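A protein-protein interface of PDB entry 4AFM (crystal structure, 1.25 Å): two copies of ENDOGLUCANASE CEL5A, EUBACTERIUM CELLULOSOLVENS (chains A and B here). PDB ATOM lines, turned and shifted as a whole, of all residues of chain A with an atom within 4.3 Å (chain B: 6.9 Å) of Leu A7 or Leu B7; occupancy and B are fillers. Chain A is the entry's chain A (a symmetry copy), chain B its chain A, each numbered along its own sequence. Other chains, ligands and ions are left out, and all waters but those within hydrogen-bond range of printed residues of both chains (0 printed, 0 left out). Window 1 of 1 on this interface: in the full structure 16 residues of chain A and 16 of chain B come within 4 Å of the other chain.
Among the printed residues, pairs that only touch across the chains: Phe A8 with Val B6, Val A6 with Phe B8, Ile A5 with Ser B9, Phe A8 with Pro B38, Pro A38 with Phe B8, Val A6 with Val B6, Ile A5 with Phe B8 and Phe A8 with Ile B5.
O of Ser B9 sits at hydrogen-bond distance from N of Val A6, at 2.8 Å.
The backbone carbonyl oxygen (O) of Leu B7 sits close to the backbone carbonyl oxygen (O) of Leu A7 (3.3 Å).
The backbone NH of Ile B5 lies within hydrogen-bond range of the backbone carbonyl oxygen of Ala B125, 2.8 Å away.
N of Leu B7 is in hydrogen-bond range of O of Ile B123, at 2.8 Å.
The backbone carbonyl oxygen of Phe B8 sits at hydrogen-bond distance from the backbone NH of Ile B123.
O of Ala A125 lies within hydrogen-bond range of N of Ile A5 (2.8 Å).
N of Leu A7 is in hydrogen-bond range of O of Ile A123 (2.8 Å).
The backbone carbonyl oxygen (O) of Phe A8 sits at hydrogen-bond distance from the backbone NH (N) of Ile A123 (2.9 Å).
Ile A5 touches Phe B8, and with the chains exchanged Phe A8 touches Ile B5.
Val A6 touches its own counterpart, Val B6.
Val A6 touches Phe B8, and with the chains exchanged Phe A8 touches Val B6.
Leu A7 touches its own counterpart, Leu B7.
9 positions are printed for both chains.
Leu A7 touches just one residue of chain B: Leu B7 (3.3 Å).
Printed residues of chain B within 4 Å of Phe A8: Ile B5 (3.8 Å), Val B6 (3.3 Å) and Pro B38 (3.7 Å).
Printed residues of chain A within 4 Å of Ile B5: Phe A8 (3.8 Å).
Phe B39 touches none of the printed residues of chain A.
The nearest printed residue of chain B that does not touch Val A6 is Leu B7 (4.4 Å).
Printed residues of chain A that touch a printed residue of chain B: Ile A5, Val A6, Leu A7, Phe A8 and Pro A38.
Of the 15 printed residues of chain B, 6 touch a printed residue of chain A.
Printed residues of chain B that touch a printed residue of chain A: Ile B5, Val B6, Leu B7, Phe B8, Ser B9 and Pro B38.
Among the printed residues, 10 pairs touch across the chains.
Among the printed residues, no Asp or Glu carboxylate lies within 4 Å of a Lys or Arg side-chain nitrogen of the other chain.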
ATOM      1  N   ILE A   5     -21.916 -16.908 -19.360  1.00  0.00           N
ATOM      2  CA  ILE A   5     -21.291 -17.862 -20.315  1.00  0.00           C
ATOM      3  C   ILE A   5     -22.056 -19.163 -20.117  1.00  0.00           C
ATOM      4  O   ILE A   5     -22.066 -19.701 -18.983  1.00  0.00           O
ATOM      5  CB  ILE A   5     -19.847 -17.971 -19.998  1.00  0.00           C
ATOM      6  CG1 ILE A   5     -19.135 -16.572 -20.132  1.00  0.00           C
ATOM      7  CG2 ILE A   5     -19.245 -19.016 -20.869  1.00  0.00           C
ATOM      8  CD1 ILE A   5     -17.751 -16.559 -19.530  1.00  0.00           C
ATOM      9  N   VAL A   6     -22.596 -19.697 -21.158  1.00  0.00           N
ATOM     10  CA  VAL A   6     -23.267 -20.997 -21.084  1.00  0.00           C
ATOM     11  C   VAL A   6     -22.225 -22.086 -21.283  1.00  0.00           C
ATOM     12  O   VAL A   6     -21.576 -22.118 -22.375  1.00  0.00           O
ATOM     13  CB  VAL A   6     -24.415 -21.097 -22.062  1.00  0.00           C
ATOM     14  CG1 VAL A   6     -25.077 -22.494 -22.012  1.00  0.00           C
ATOM     15  CG2 VAL A   6     -25.439 -19.995 -21.846  1.00  0.00           C
ATOM     16  N   LEU A   7     -21.983 -22.904 -20.291  1.00  0.00           N
ATOM     17  CA  LEU A   7     -21.076 -24.049 -20.380  1.00  0.00           C
ATOM     18  C   LEU A   7     -21.772 -25.247 -20.895  1.00  0.00           C
ATOM     19  O   LEU A   7     -21.102 -26.170 -21.418  1.00  0.00           O
ATOM     20  CB  LEU A   7     -20.459 -24.320 -18.983  1.00  0.00           C
ATOM     21  CG  LEU A   7     -19.709 -23.171 -18.385  1.00  0.00           C
ATOM     22  CD1 LEU A   7     -19.067 -23.560 -17.041  1.00  0.00           C
ATOM     23  CD2 LEU A   7     -18.716 -22.582 -19.287  1.00  0.00           C
ATOM     24  N   PHE A   8     -23.074 -25.342 -20.748  1.00  0.00           N
ATOM     25  CA  PHE A   8     -23.886 -26.460 -21.228  1.00  0.00           C
ATOM     26  C   PHE A   8     -25.325 -26.049 -21.205  1.00  0.00           C
ATOM     27  O   PHE A   8     -25.784 -25.455 -20.186  1.00  0.00           O
ATOM     28  CB  PHE A   8     -23.737 -27.694 -20.281  1.00  0.00           C
ATOM     29  CG  PHE A   8     -24.645 -28.819 -20.672  1.00  0.00           C
ATOM     30  CD1 PHE A   8     -24.354 -29.632 -21.790  1.00  0.00           C
ATOM     31  CD2 PHE A   8     -25.838 -29.047 -19.985  1.00  0.00           C
ATOM     32  CE1 PHE A   8     -25.245 -30.616 -22.150  1.00  0.00           C
ATOM     33  CE2 PHE A   8     -26.736 -30.048 -20.363  1.00  0.00           C
ATOM     34  CZ  PHE A   8     -26.393 -30.869 -21.459  1.00  0.00           C
ATOM     35  N   TYR A  28     -20.634 -32.942 -15.860  1.00  0.00           N
ATOM     36  CA  TYR A  28     -19.831 -31.986 -16.610  1.00  0.00           C
ATOM     37  C   TYR A  28     -18.424 -32.026 -16.051  1.00  0.00           C
ATOM     38  O   TYR A  28     -18.298 -32.079 -14.785  1.00  0.00           O
ATOM     39  CB  TYR A  28     -20.430 -30.560 -16.339  1.00  0.00           C
ATOM     40  CG  TYR A  28     -19.657 -29.448 -17.005  1.00  0.00           C
ATOM     41  CD1 TYR A  28     -19.910 -29.066 -18.313  1.00  0.00           C
ATOM     42  CD2 TYR A  28     -18.669 -28.742 -16.298  1.00  0.00           C
ATOM     43  CE1 TYR A  28     -19.180 -28.043 -18.963  1.00  0.00           C
ATOM     44  CE2 TYR A  28     -17.929 -27.748 -16.890  1.00  0.00           C
ATOM     45  CZ  TYR A  28     -18.183 -27.408 -18.194  1.00  0.00           C
ATOM     46  OH  TYR A  28     -17.492 -26.363 -18.837  1.00  0.00           O
ATOM     47  N   PRO A  38     -13.510 -22.272 -21.086  1.00  0.00           N
ATOM     48  CA  PRO A  38     -14.651 -21.499 -21.511  1.00  0.00           C
ATOM     49  C   PRO A  38     -14.902 -20.269 -20.696  1.00  0.00           C
ATOM     50  O   PRO A  38     -15.684 -19.373 -21.097  1.00  0.00           O
ATOM     51  CB  PRO A  38     -15.808 -22.506 -21.442  1.00  0.00           C
ATOM     52  CG  PRO A  38     -15.411 -23.401 -20.302  1.00  0.00           C
ATOM     53  CD  PRO A  38     -13.919 -23.591 -20.490  1.00  0.00           C
ATOM     54  N   PHE A  39     -14.303 -20.141 -19.492  1.00  0.00           N
ATOM     55  CA  PHE A  39     -14.438 -18.967 -18.673  1.00  0.00           C
ATOM     56  C   PHE A  39     -13.087 -18.742 -18.003  1.00  0.00           C
ATOM     57  O   PHE A  39     -12.231 -19.629 -17.949  1.00  0.00           O
ATOM     58  CB  PHE A  39     -15.607 -19.019 -17.682  1.00  0.00           C
ATOM     59  CG  PHE A  39     -15.416 -19.950 -16.536  1.00  0.00           C
ATOM     60  CD1 PHE A  39     -15.599 -21.328 -16.661  1.00  0.00           C
ATOM     61  CD2 PHE A  39     -14.997 -19.478 -15.293  1.00  0.00           C
ATOM     62  CE1 PHE A  39     -15.425 -22.198 -15.588  1.00  0.00           C
ATOM     63  CE2 PHE A  39     -14.870 -20.350 -14.237  1.00  0.00           C
ATOM     64  CZ  PHE A  39     -15.010 -21.709 -14.383  1.00  0.00           C
ATOM     65  N   ILE A 123     -25.751 -25.148 -17.351  1.00  0.00           N
ATOM     66  CA  ILE A 123     -24.622 -24.745 -16.502  1.00  0.00           C
ATOM     67  C   ILE A 123     -24.138 -23.432 -17.034  1.00  0.00           C
ATOM     68  O   ILE A 123     -23.846 -23.317 -18.249  1.00  0.00           O
ATOM     69  CB  ILE A 123     -23.483 -25.773 -16.518  1.00  0.00           C
ATOM     70  CG1 ILE A 123     -23.969 -27.172 -16.116  1.00  0.00           C
ATOM     71  CG2 ILE A 123     -22.344 -25.316 -15.652  1.00  0.00           C
ATOM     72  CD1 ILE A 123     -22.918 -28.274 -16.223  1.00  0.00           C
ATOM     73  N   ALA A 125     -21.519 -19.979 -16.185  1.00  0.00           N
ATOM     74  CA  ALA A 125     -20.546 -19.187 -15.396  1.00  0.00           C
ATOM     75  C   ALA A 125     -20.918 -17.749 -15.554  1.00  0.00           C
ATOM     76  O   ALA A 125     -21.093 -17.236 -16.669  1.00  0.00           O
ATOM     77  CB  ALA A 125     -19.126 -19.413 -15.877  1.00  0.00           C
ATOM     78  N   ILE B   5     -28.275 -28.834 -28.360  1.00  0.00           N
ATOM     79  CA  ILE B   5     -27.448 -28.867 -27.124  1.00  0.00           C
ATOM     80  C   ILE B   5     -26.473 -27.709 -27.280  1.00  0.00           C
ATOM     81  O   ILE B   5     -25.697 -27.692 -28.266  1.00  0.00           O
ATOM     82  CB  ILE B   5     -26.785 -30.189 -27.032  1.00  0.00           C
ATOM     83  CG1 ILE B   5     -27.850 -31.348 -26.967  1.00  0.00           C
ATOM     84  CG2 ILE B   5     -25.862 -30.181 -25.866  1.00  0.00           C
ATOM     85  CD1 ILE B   5     -27.243 -32.714 -27.183  1.00  0.00           C
ATOM     86  N   VAL B   6     -26.439 -26.831 -26.338  1.00  0.00           N
ATOM     87  CA  VAL B   6     -25.466 -25.737 -26.353  1.00  0.00           C
ATOM     88  C   VAL B   6     -24.182 -26.227 -25.703  1.00  0.00           C
ATOM     89  O   VAL B   6     -24.219 -26.612 -24.493  1.00  0.00           O
ATOM     90  CB  VAL B   6     -26.012 -24.486 -25.703  1.00  0.00           C
ATOM     91  CG1 VAL B   6     -24.954 -23.357 -25.677  1.00  0.00           C
ATOM     92  CG2 VAL B   6     -27.297 -24.019 -26.367  1.00  0.00           C
ATOM     93  N   LEU B   7     -23.104 -26.306 -26.441  1.00  0.00           N
ATOM     94  CA  LEU B   7     -21.786 -26.673 -25.920  1.00  0.00           C
ATOM     95  C   LEU B   7     -21.065 -25.491 -25.400  1.00  0.00           C
ATOM     96  O   LEU B   7     -20.140 -25.653 -24.569  1.00  0.00           O
ATOM     97  CB  LEU B   7     -20.973 -27.374 -27.040  1.00  0.00           C
ATOM     98  CG  LEU B   7     -21.609 -28.600 -27.616  1.00  0.00           C
ATOM     99  CD1 LEU B   7     -20.695 -29.268 -28.659  1.00  0.00           C
ATOM    100  CD2 LEU B   7     -22.044 -29.568 -26.606  1.00  0.00           C
ATOM    101  N   PHE B   8     -21.376 -24.301 -25.860  1.00  0.00           N
ATOM    102  CA  PHE B   8     -20.759 -23.051 -25.418  1.00  0.00           C
ATOM    103  C   PHE B   8     -21.606 -21.909 -25.883  1.00  0.00           C
ATOM    104  O   PHE B   8     -22.034 -21.899 -27.074  1.00  0.00           O
ATOM    105  CB  PHE B   8     -19.346 -22.878 -26.062  1.00  0.00           C
ATOM    106  CG  PHE B   8     -18.730 -21.554 -25.728  1.00  0.00           C
ATOM    107  CD1 PHE B   8     -18.185 -21.309 -24.447  1.00  0.00           C
ATOM    108  CD2 PHE B   8     -18.746 -20.505 -26.649  1.00  0.00           C
ATOM    109  CE1 PHE B   8     -17.684 -20.060 -24.163  1.00  0.00           C
ATOM    110  CE2 PHE B   8     -18.235 -19.241 -26.346  1.00  0.00           C
ATOM    111  CZ  PHE B   8     -17.660 -19.043 -25.072  1.00  0.00           C
ATOM    112  N   SER B   9     -21.815 -20.863 -25.077  1.00  0.00           N
ATOM    113  CA  SER B   9     -22.236 -19.591 -25.661  1.00  0.00           C
ATOM    114  C   SER B   9     -21.607 -18.489 -24.801  1.00  0.00           C
ATOM    115  O   SER B   9     -21.579 -18.580 -23.561  1.00  0.00           O
ATOM    116  CB  SER B   9     -23.733 -19.524 -25.851  1.00  0.00           C
ATOM    117  OG  SER B   9     -24.278 -19.273 -24.635  1.00  0.00           O
ATOM    118  N   TYR B  28     -12.409 -24.450 -28.539  1.00  0.00           N
ATOM    119  CA  TYR B  28     -13.202 -25.413 -27.787  1.00  0.00           C
ATOM    120  C   TYR B  28     -12.551 -26.771 -27.947  1.00  0.00           C
ATOM    121  O   TYR B  28     -12.133 -27.088 -29.108  1.00  0.00           O
ATOM    122  CB  TYR B  28     -14.624 -25.466 -28.449  1.00  0.00           C
ATOM    123  CG  TYR B  28     -15.546 -26.477 -27.812  1.00  0.00           C
ATOM    124  CD1 TYR B  28     -16.315 -26.165 -26.702  1.00  0.00           C
ATOM    125  CD2 TYR B  28     -15.673 -27.768 -28.353  1.00  0.00           C
ATOM    126  CE1 TYR B  28     -17.166 -27.105 -26.076  1.00  0.00           C
ATOM    127  CE2 TYR B  28     -16.479 -28.716 -27.774  1.00  0.00           C
ATOM    128  CZ  TYR B  28     -17.209 -28.388 -26.659  1.00  0.00           C
ATOM    129  OH  TYR B  28     -18.092 -29.304 -26.053  1.00  0.00           O
ATOM    130  N   LEU B  30     -12.620 -31.078 -26.582  1.00  0.00           N
ATOM    131  CA  LEU B  30     -13.117 -32.185 -25.745  1.00  0.00           C
ATOM    132  C   LEU B  30     -12.255 -33.347 -25.905  1.00  0.00           C
ATOM    133  O   LEU B  30     -11.643 -33.627 -27.061  1.00  0.00           O
ATOM    134  CB  LEU B  30     -14.415 -32.758 -26.179  1.00  0.00           C
ATOM    135  CG  LEU B  30     -15.515 -31.842 -26.075  1.00  0.00           C
ATOM    136  CD1 LEU B  30     -16.890 -32.434 -26.695  1.00  0.00           C
ATOM    137  CD2 LEU B  30     -16.019 -31.718 -24.584  1.00  0.00           C
ATOM    138  N   MET B  37     -19.429 -36.728 -21.811  1.00  0.00           N
ATOM    139  CA  MET B  37     -19.765 -36.101 -23.088  1.00  0.00           C
ATOM    140  C   MET B  37     -21.026 -35.257 -22.994  1.00  0.00           C
ATOM    141  O   MET B  37     -22.040 -35.715 -22.453  1.00  0.00           O
ATOM    142  CB  MET B  37     -19.973 -37.256 -24.105  1.00  0.00           C
ATOM    143  CG  MET B  37     -18.681 -37.870 -24.616  1.00  0.00           C
ATOM    144  SD  MET B  37     -17.556 -36.542 -25.609  1.00  0.00           S
ATOM    145  CE  MET B  37     -18.820 -36.326 -27.130  1.00  0.00           C
ATOM    146  N   PRO B  38     -21.050 -34.089 -23.606  1.00  0.00           N
ATOM    147  CA  PRO B  38     -22.242 -33.278 -23.634  1.00  0.00           C
ATOM    148  C   PRO B  38     -23.230 -33.666 -24.689  1.00  0.00           C
ATOM    149  O   PRO B  38     -24.407 -33.231 -24.666  1.00  0.00           O
ATOM    150  CB  PRO B  38     -21.698 -31.854 -23.821  1.00  0.00           C
ATOM    151  CG  PRO B  38     -20.460 -32.071 -24.644  1.00  0.00           C
ATOM    152  CD  PRO B  38     -19.838 -33.317 -24.047  1.00  0.00           C
ATOM    153  N   PHE B  39     -22.835 -34.469 -25.699  1.00  0.00           N
ATOM    154  CA  PHE B  39     -23.733 -34.942 -26.719  1.00  0.00           C
ATOM    155  C   PHE B  39     -23.311 -36.371 -27.045  1.00  0.00           C
ATOM    156  O   PHE B  39     -22.207 -36.815 -26.720  1.00  0.00           O
ATOM    157  CB  PHE B  39     -23.820 -34.037 -27.954  1.00  0.00           C
ATOM    158  CG  PHE B  39     -22.616 -34.053 -28.829  1.00  0.00           C
ATOM    159  CD1 PHE B  39     -21.460 -33.335 -28.516  1.00  0.00           C
ATOM    160  CD2 PHE B  39     -22.583 -34.833 -29.984  1.00  0.00           C
ATOM    161  CE1 PHE B  39     -20.336 -33.347 -29.337  1.00  0.00           C
ATOM    162  CE2 PHE B  39     -21.476 -34.798 -30.801  1.00  0.00           C
ATOM    163  CZ  PHE B  39     -20.330 -34.123 -30.460  1.00  0.00           C
ATOM    164  N   ILE B  47     -22.620 -30.114 -35.958  1.00  0.00           N
ATOM    165  CA  ILE B  47     -22.075 -29.127 -35.030  1.00  0.00           C
ATOM    166  C   ILE B  47     -22.163 -27.769 -35.701  1.00  0.00           C
ATOM    167  O   ILE B  47     -21.669 -27.646 -36.889  1.00  0.00           O
ATOM    168  CB  ILE B  47     -20.623 -29.513 -34.689  1.00  0.00           C
ATOM    169  CG1 ILE B  47     -20.626 -30.854 -33.861  1.00  0.00           C
ATOM    170  CG2 ILE B  47     -19.914 -28.386 -33.881  1.00  0.00           C
ATOM    171  CD1 ILE B  47     -19.285 -31.417 -33.668  1.00  0.00           C
ATOM    172  N   LYS B 122     -20.996 -19.062 -30.101  1.00  0.00           N
ATOM    173  CA  LYS B 122     -21.915 -20.163 -29.781  1.00  0.00           C
ATOM    174  C   LYS B 122     -21.459 -21.422 -30.476  1.00  0.00           C
ATOM    175  O   LYS B 122     -21.012 -21.350 -31.634  1.00  0.00           O
ATOM    176  CB  LYS B 122     -23.338 -19.784 -30.197  1.00  0.00           C
ATOM    177  CG  LYS B 122     -24.345 -20.706 -29.563  1.00  0.00           C
ATOM    178  CD  LYS B 122     -25.796 -20.171 -29.836  1.00  0.00           C
ATOM    179  CE  LYS B 122     -26.781 -20.863 -28.963  1.00  0.00           C
ATOM    180  NZ  LYS B 122     -28.207 -20.352 -29.092  1.00  0.00           N
ATOM    181  N   ILE B 123     -21.569 -22.545 -29.813  1.00  0.00           N
ATOM    182  CA  ILE B 123     -21.338 -23.872 -30.398  1.00  0.00           C
ATOM    183  C   ILE B 123     -22.504 -24.722 -29.998  1.00  0.00           C
ATOM    184  O   ILE B 123     -22.824 -24.817 -28.788  1.00  0.00           O
ATOM    185  CB  ILE B 123     -20.030 -24.507 -29.908  1.00  0.00           C
ATOM    186  CG1 ILE B 123     -18.820 -23.599 -30.170  1.00  0.00           C
ATOM    187  CG2 ILE B 123     -19.839 -25.867 -30.517  1.00  0.00           C
ATOM    188  CD1 ILE B 123     -17.498 -24.109 -29.604  1.00  0.00           C
ATOM    189  N   VAL B 124     -23.160 -25.312 -30.976  1.00  0.00           N
ATOM    190  CA  VAL B 124     -24.319 -26.213 -30.672  1.00  0.00           C
ATOM    191  C   VAL B 124     -24.168 -27.496 -31.390  1.00  0.00           C
ATOM    192  O   VAL B 124     -23.601 -27.613 -32.521  1.00  0.00           O
ATOM    193  CB  VAL B 124     -25.624 -25.577 -31.118  1.00  0.00           C
ATOM    194  CG1 VAL B 124     -25.867 -24.297 -30.412  1.00  0.00           C
ATOM    195  CG2 VAL B 124     -25.659 -25.430 -32.545  1.00  0.00           C
ATOM    196  N   ALA B 125     -24.539 -28.572 -30.734  1.00  0.00           N
ATOM    197  CA  ALA B 125     -24.727 -29.897 -31.372  1.00  0.00           C
ATOM    198  C   ALA B 125     -26.196 -30.084 -31.570  1.00  0.00           C
ATOM    199  O   ALA B 125     -27.008 -29.927 -30.646  1.00  0.00           O
ATOM    200  CB  ALA B 125     -24.172 -31.012 -30.508  1.00  0.00           C
